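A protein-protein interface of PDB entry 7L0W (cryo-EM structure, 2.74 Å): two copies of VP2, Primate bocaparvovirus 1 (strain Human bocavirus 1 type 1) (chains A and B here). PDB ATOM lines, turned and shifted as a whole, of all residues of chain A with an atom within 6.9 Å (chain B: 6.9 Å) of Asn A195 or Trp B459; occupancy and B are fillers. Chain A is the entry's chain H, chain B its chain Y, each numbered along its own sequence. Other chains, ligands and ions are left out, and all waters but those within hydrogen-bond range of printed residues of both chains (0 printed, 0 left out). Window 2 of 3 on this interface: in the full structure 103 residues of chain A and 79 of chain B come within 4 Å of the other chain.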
ATOM      1  N   TYR A  40     -31.306  -7.921  -2.825  1.00  0.00           N
ATOM      2  CA  TYR A  40     -30.657  -9.217  -2.905  1.00  0.00           C
ATOM      3  C   TYR A  40     -30.039  -9.511  -1.549  1.00  0.00           C
ATOM      4  O   TYR A  40     -29.450  -8.622  -0.930  1.00  0.00           O
ATOM      5  CB  TYR A  40     -29.592  -9.227  -3.990  1.00  0.00           C
ATOM      6  CG  TYR A  40     -30.130  -9.162  -5.389  1.00  0.00           C
ATOM      7  CD1 TYR A  40     -30.241 -10.293  -6.164  1.00  0.00           C
ATOM      8  CD2 TYR A  40     -30.568  -7.974  -5.919  1.00  0.00           C
ATOM      9  CE1 TYR A  40     -30.729 -10.227  -7.439  1.00  0.00           C
ATOM     10  CE2 TYR A  40     -31.069  -7.907  -7.183  1.00  0.00           C
ATOM     11  CZ  TYR A  40     -31.146  -9.033  -7.936  1.00  0.00           C
ATOM     12  OH  TYR A  40     -31.646  -8.955  -9.210  1.00  0.00           O
ATOM     13  N   TYR A 133     -28.606 -17.117 -16.177  1.00  0.00           N
ATOM     14  CA  TYR A 133     -28.844 -17.087 -14.744  1.00  0.00           C
ATOM     15  C   TYR A 133     -29.186 -18.476 -14.242  1.00  0.00           C
ATOM     16  O   TYR A 133     -29.606 -19.341 -15.007  1.00  0.00           O
ATOM     17  CB  TYR A 133     -29.947 -16.089 -14.440  1.00  0.00           C
ATOM     18  CG  TYR A 133     -29.596 -14.696 -14.882  1.00  0.00           C
ATOM     19  CD1 TYR A 133     -28.787 -13.892 -14.111  1.00  0.00           C
ATOM     20  CD2 TYR A 133     -30.079 -14.190 -16.070  1.00  0.00           C
ATOM     21  CE1 TYR A 133     -28.461 -12.634 -14.514  1.00  0.00           C
ATOM     22  CE2 TYR A 133     -29.756 -12.930 -16.478  1.00  0.00           C
ATOM     23  CZ  TYR A 133     -28.948 -12.155 -15.695  1.00  0.00           C
ATOM     24  OH  TYR A 133     -28.625 -10.886 -16.100  1.00  0.00           O
ATOM     25  N   PRO A 189     -20.223 -17.172  -7.259  1.00  0.00           N
ATOM     26  CA  PRO A 189     -20.855 -16.268  -8.217  1.00  0.00           C
ATOM     27  C   PRO A 189     -22.026 -15.537  -7.599  1.00  0.00           C
ATOM     28  O   PRO A 189     -22.693 -16.043  -6.698  1.00  0.00           O
ATOM     29  CB  PRO A 189     -21.312 -17.208  -9.330  1.00  0.00           C
ATOM     30  CG  PRO A 189     -21.523 -18.459  -8.647  1.00  0.00           C
ATOM     31  CD  PRO A 189     -20.449 -18.570  -7.624  1.00  0.00           C
ATOM     32  N   PHE A 190     -22.257 -14.326  -8.085  1.00  0.00           N
ATOM     33  CA  PHE A 190     -23.370 -13.499  -7.657  1.00  0.00           C
ATOM     34  C   PHE A 190     -24.066 -12.970  -8.893  1.00  0.00           C
ATOM     35  O   PHE A 190     -23.471 -12.215  -9.664  1.00  0.00           O
ATOM     36  CB  PHE A 190     -22.884 -12.360  -6.776  1.00  0.00           C
ATOM     37  CG  PHE A 190     -23.935 -11.364  -6.434  1.00  0.00           C
ATOM     38  CD1 PHE A 190     -25.009 -11.718  -5.665  1.00  0.00           C
ATOM     39  CD2 PHE A 190     -23.796 -10.052  -6.799  1.00  0.00           C
ATOM     40  CE1 PHE A 190     -25.960 -10.804  -5.342  1.00  0.00           C
ATOM     41  CE2 PHE A 190     -24.743  -9.136  -6.462  1.00  0.00           C
ATOM     42  CZ  PHE A 190     -25.820  -9.514  -5.729  1.00  0.00           C
ATOM     43  N   PHE A 191     -25.314 -13.366  -9.084  1.00  0.00           N
ATOM     44  CA  PHE A 191     -26.055 -13.021 -10.281  1.00  0.00           C
ATOM     45  C   PHE A 191     -27.104 -11.976  -9.951  1.00  0.00           C
ATOM     46  O   PHE A 191     -27.871 -12.138  -9.000  1.00  0.00           O
ATOM     47  CB  PHE A 191     -26.710 -14.259 -10.882  1.00  0.00           C
ATOM     48  CG  PHE A 191     -25.736 -15.305 -11.299  1.00  0.00           C
ATOM     49  CD1 PHE A 191     -25.106 -15.230 -12.518  1.00  0.00           C
ATOM     50  CD2 PHE A 191     -25.447 -16.361 -10.472  1.00  0.00           C
ATOM     51  CE1 PHE A 191     -24.214 -16.186 -12.894  1.00  0.00           C
ATOM     52  CE2 PHE A 191     -24.556 -17.316 -10.848  1.00  0.00           C
ATOM     53  CZ  PHE A 191     -23.938 -17.229 -12.058  1.00  0.00           C
ATOM     54  N   LEU A 192     -27.120 -10.904 -10.727  1.00  0.00           N
ATOM     55  CA  LEU A 192     -28.171  -9.907 -10.684  1.00  0.00           C
ATOM     56  C   LEU A 192     -28.971  -9.992 -11.968  1.00  0.00           C
ATOM     57  O   LEU A 192     -28.407  -9.935 -13.060  1.00  0.00           O
ATOM     58  CB  LEU A 192     -27.609  -8.502 -10.553  1.00  0.00           C
ATOM     59  CG  LEU A 192     -26.818  -8.198  -9.301  1.00  0.00           C
ATOM     60  CD1 LEU A 192     -26.350  -6.781  -9.346  1.00  0.00           C
ATOM     61  CD2 LEU A 192     -27.717  -8.406  -8.149  1.00  0.00           C
ATOM     62  N   LEU A 193     -30.282 -10.121 -11.844  1.00  0.00           N
ATOM     63  CA  LEU A 193     -31.109 -10.092 -13.036  1.00  0.00           C
ATOM     64  C   LEU A 193     -31.095  -8.733 -13.720  1.00  0.00           C
ATOM     65  O   LEU A 193     -31.653  -8.605 -14.812  1.00  0.00           O
ATOM     66  CB  LEU A 193     -32.540 -10.482 -12.688  1.00  0.00           C
ATOM     67  CG  LEU A 193     -32.964 -11.946 -12.626  1.00  0.00           C
ATOM     68  CD1 LEU A 193     -32.838 -12.582 -13.961  1.00  0.00           C
ATOM     69  CD2 LEU A 193     -32.176 -12.702 -11.596  1.00  0.00           C
ATOM     70  N   GLU A 194     -30.485  -7.720 -13.102  1.00  0.00           N
ATOM     71  CA  GLU A 194     -30.422  -6.400 -13.717  1.00  0.00           C
ATOM     72  C   GLU A 194     -29.297  -6.300 -14.732  1.00  0.00           C
ATOM     73  O   GLU A 194     -29.289  -5.386 -15.560  1.00  0.00           O
ATOM     74  CB  GLU A 194     -30.265  -5.332 -12.647  1.00  0.00           C
ATOM     75  CG  GLU A 194     -31.498  -5.111 -11.826  1.00  0.00           C
ATOM     76  CD  GLU A 194     -31.670  -6.126 -10.738  1.00  0.00           C
ATOM     77  OE1 GLU A 194     -30.852  -7.060 -10.649  1.00  0.00           O
ATOM     78  OE2 GLU A 194     -32.634  -5.994  -9.967  1.00  0.00           O
ATOM     79  N   ASN A 195     -28.327  -7.209 -14.676  1.00  0.00           N
ATOM     80  CA  ASN A 195     -27.291  -7.230 -15.702  1.00  0.00           C
ATOM     81  C   ASN A 195     -27.895  -7.272 -17.093  1.00  0.00           C
ATOM     82  O   ASN A 195     -27.541  -6.471 -17.951  1.00  0.00           O
ATOM     83  CB  ASN A 195     -26.369  -8.425 -15.507  1.00  0.00           C
ATOM     84  CG  ASN A 195     -25.466  -8.266 -14.324  1.00  0.00           C
ATOM     85  OD1 ASN A 195     -25.205  -7.151 -13.884  1.00  0.00           O
ATOM     86  ND2 ASN A 195     -24.974  -9.380 -13.800  1.00  0.00           N
ATOM     87  N   SER A 196     -28.800  -8.200 -17.338  1.00  0.00           N
ATOM     88  CA  SER A 196     -29.354  -8.377 -18.665  1.00  0.00           C
ATOM     89  C   SER A 196     -30.357  -7.281 -19.010  1.00  0.00           C
ATOM     90  O   SER A 196     -30.895  -6.601 -18.135  1.00  0.00           O
ATOM     91  CB  SER A 196     -30.009  -9.746 -18.757  1.00  0.00           C
ATOM     92  OG  SER A 196     -30.955  -9.881 -17.719  1.00  0.00           O
ATOM     93  N   ASP A 197     -30.584  -7.106 -20.308  1.00  0.00           N
ATOM     94  CA  ASP A 197     -31.636  -6.222 -20.781  1.00  0.00           C
ATOM     95  C   ASP A 197     -32.985  -6.894 -20.595  1.00  0.00           C
ATOM     96  O   ASP A 197     -33.131  -8.092 -20.836  1.00  0.00           O
ATOM     97  CB  ASP A 197     -31.448  -5.899 -22.261  1.00  0.00           C
ATOM     98  CG  ASP A 197     -30.164  -5.157 -22.542  1.00  0.00           C
ATOM     99  OD1 ASP A 197     -29.519  -4.706 -21.583  1.00  0.00           O
ATOM    100  OD2 ASP A 197     -29.805  -5.009 -23.729  1.00  0.00           O
ATOM    101  N   HIS A 198     -33.983  -6.122 -20.183  1.00  0.00           N
ATOM    102  CA  HIS A 198     -35.328  -6.660 -20.097  1.00  0.00           C
ATOM    103  C   HIS A 198     -36.345  -5.548 -20.264  1.00  0.00           C
ATOM    104  O   HIS A 198     -36.016  -4.364 -20.267  1.00  0.00           O
ATOM    105  CB  HIS A 198     -35.580  -7.427 -18.800  1.00  0.00           C
ATOM    106  CG  HIS A 198     -35.335  -6.648 -17.551  1.00  0.00           C
ATOM    107  ND1 HIS A 198     -34.116  -6.632 -16.913  1.00  0.00           N
ATOM    108  CD2 HIS A 198     -36.151  -5.857 -16.820  1.00  0.00           C
ATOM    109  CE1 HIS A 198     -34.199  -5.880 -15.831  1.00  0.00           C
ATOM    110  NE2 HIS A 198     -35.420  -5.391 -15.757  1.00  0.00           N
ATOM    111  N   THR B 456     -20.325 -14.050 -19.461  1.00  0.00           N
ATOM    112  CA  THR B 456     -20.999 -14.384 -18.220  1.00  0.00           C
ATOM    113  C   THR B 456     -21.841 -13.215 -17.746  1.00  0.00           C
ATOM    114  O   THR B 456     -21.541 -12.055 -18.035  1.00  0.00           O
ATOM    115  CB  THR B 456     -20.005 -14.767 -17.126  1.00  0.00           C
ATOM    116  OG1 THR B 456     -20.719 -15.176 -15.956  1.00  0.00           O
ATOM    117  CG2 THR B 456     -19.125 -13.601 -16.782  1.00  0.00           C
ATOM    118  N   LYS B 457     -22.919 -13.537 -17.040  1.00  0.00           N
ATOM    119  CA  LYS B 457     -23.716 -12.539 -16.350  1.00  0.00           C
ATOM    120  C   LYS B 457     -23.346 -12.429 -14.882  1.00  0.00           C
ATOM    121  O   LYS B 457     -23.976 -11.661 -14.154  1.00  0.00           O
ATOM    122  CB  LYS B 457     -25.203 -12.852 -16.480  1.00  0.00           C
ATOM    123  CG  LYS B 457     -25.677 -13.035 -17.898  1.00  0.00           C
ATOM    124  CD  LYS B 457     -25.308 -11.876 -18.791  1.00  0.00           C
ATOM    125  CE  LYS B 457     -26.164 -10.666 -18.558  1.00  0.00           C
ATOM    126  NZ  LYS B 457     -25.840  -9.619 -19.556  1.00  0.00           N
ATOM    127  N   ASN B 458     -22.356 -13.190 -14.432  1.00  0.00           N
ATOM    128  CA  ASN B 458     -21.887 -13.100 -13.059  1.00  0.00           C
ATOM    129  C   ASN B 458     -21.458 -11.677 -12.747  1.00  0.00           C
ATOM    130  O   ASN B 458     -20.843 -11.010 -13.582  1.00  0.00           O
ATOM    131  CB  ASN B 458     -20.733 -14.063 -12.838  1.00  0.00           C
ATOM    132  CG  ASN B 458     -20.290 -14.108 -11.410  1.00  0.00           C
ATOM    133  OD1 ASN B 458     -21.076 -13.865 -10.506  1.00  0.00           O
ATOM    134  ND2 ASN B 458     -19.027 -14.420 -11.191  1.00  0.00           N
ATOM    135  N   TRP B 459     -21.802 -11.205 -11.552  1.00  0.00           N
ATOM    136  CA  TRP B 459     -21.436  -9.853 -11.153  1.00  0.00           C
ATOM    137  C   TRP B 459     -20.010  -9.800 -10.636  1.00  0.00           C
ATOM    138  O   TRP B 459     -19.243  -8.898 -10.980  1.00  0.00           O
ATOM    139  CB  TRP B 459     -22.407  -9.363 -10.085  1.00  0.00           C
ATOM    140  CG  TRP B 459     -22.124  -8.024  -9.570  1.00  0.00           C
ATOM    141  CD1 TRP B 459     -21.514  -7.715  -8.404  1.00  0.00           C
ATOM    142  CD2 TRP B 459     -22.477  -6.789 -10.181  1.00  0.00           C
ATOM    143  NE1 TRP B 459     -21.442  -6.359  -8.254  1.00  0.00           N
ATOM    144  CE2 TRP B 459     -22.032  -5.768  -9.336  1.00  0.00           C
ATOM    145  CE3 TRP B 459     -23.119  -6.448 -11.367  1.00  0.00           C
ATOM    146  CZ2 TRP B 459     -22.206  -4.437  -9.637  1.00  0.00           C
ATOM    147  CZ3 TRP B 459     -23.291  -5.133 -11.661  1.00  0.00           C
ATOM    148  CH2 TRP B 459     -22.837  -4.140 -10.805  1.00  0.00           C
ATOM    149  N   ARG B 460     -19.634 -10.776  -9.828  1.00  0.00           N
ATOM    150  CA  ARG B 460     -18.410 -10.749  -9.062  1.00  0.00           C
ATOM    151  C   ARG B 460     -17.180 -11.005  -9.918  1.00  0.00           C
ATOM    152  O   ARG B 460     -17.283 -11.412 -11.073  1.00  0.00           O
ATOM    153  CB  ARG B 460     -18.487 -11.795  -7.965  1.00  0.00           C
ATOM    154  CG  ARG B 460     -19.269 -11.401  -6.774  1.00  0.00           C
ATOM    155  CD  ARG B 460     -19.280 -12.564  -5.847  1.00  0.00           C
ATOM    156  NE  ARG B 460     -17.943 -13.134  -5.760  1.00  0.00           N
ATOM    157  CZ  ARG B 460     -16.979 -12.653  -5.000  1.00  0.00           C
ATOM    158  NH1 ARG B 460     -17.199 -11.597  -4.266  1.00  0.00           N
ATOM    159  NH2 ARG B 460     -15.793 -13.217  -4.982  1.00  0.00           N
ATOM    160  N   PRO B 461     -15.992 -10.770  -9.371  1.00  0.00           N
ATOM    161  CA  PRO B 461     -14.782 -11.225 -10.043  1.00  0.00           C
ATOM    162  C   PRO B 461     -14.676 -12.735 -10.010  1.00  0.00           C
ATOM    163  O   PRO B 461     -15.299 -13.405  -9.187  1.00  0.00           O
ATOM    164  CB  PRO B 461     -13.664 -10.585  -9.222  1.00  0.00           C
ATOM    165  CG  PRO B 461     -14.284  -9.438  -8.598  1.00  0.00           C
ATOM    166  CD  PRO B 461     -15.664  -9.869  -8.261  1.00  0.00           C
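The side-chain amide nitrogen (ND2) of Asn A195 is in hydrogen-bond range of the backbone carbonyl oxygen (O) of Lys B457, at 2.5 Å. The backbone NH of Phe A190 lies within hydrogen-bond range of the side-chain amide oxygen of Asn B458 (2.7 Å). The backbone carbonyl oxygen (O) of Phe A190 is in hydrogen-bond range of the backbone NH (N) of Trp B459.
OD1 of Asn B458 is in hydrogen-bond range of N of Arg B460, 3.5 Å away. OG1 of Thr B456 is in hydrogen-bond range of N of Asn B458 (3.0 Å). The side-chain hydroxyl of Tyr A133 lies within hydrogen-bond range of the backbone NH of Ser A196 (3.0 Å). O of Ser A196 is in hydrogen-bond range of ND1 of His A198, at 3.4 Å. The side-chain hydroxyl of Tyr A133 lies close to the backbone carbonyl oxygen of Leu A192 (3.2 Å). The side-chain hydroxyl of Ser A196 lies within hydrogen-bond range of the backbone carbonyl oxygen of Leu A193, 3.3 Å away.
OH of Tyr A133 touches CE of Lys B457, 3.5 Å away. Pro A189 touches Asn B458. CB of Phe A190 touches CD of Arg B460, 3.7 Å away. Asn B458 touches Phe A191 (N to CE1, 3.8 Å). Trp B459 touches Leu A192. Asn A195 touches Trp B459 (OD1 to CE3, 3.3 Å). Lys B457 touches Ser A196.
Of the printed residues of chain B, Pro A189 touches Asn B458 (3.3 Å). Leu A193 touches none of the printed residues of chain B. Of chain B, only Lys B457 and Trp B459 come within 4 Å of Asn A195. Of chain A, only Phe A190, Leu A192 and Asn A195 come within 4 Å of Trp B459. Of the printed residues of chain A, Arg B460 touches Phe A190 (3.7 Å). The nearest residue of chain A that does not touch Trp B459 is Phe A191 (4.8 Å).
Hydrophobic or aromatic side chains of chain A within 4 Å of the printed part of chain B: Tyr A133, Pro A189, Phe A190, Phe A191 and Leu A192. Of the 6 printed residues of chain B, 4 touch a printed residue of chain A. Hydrophobic or aromatic side chains of chain B that line the printed part of chain A: Trp B459. Among the printed residues, no Asp or Glu carboxylate lies within 4 Å of a Lys or Arg side-chain nitrogen of the other chain.
No position is printed for both chains.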
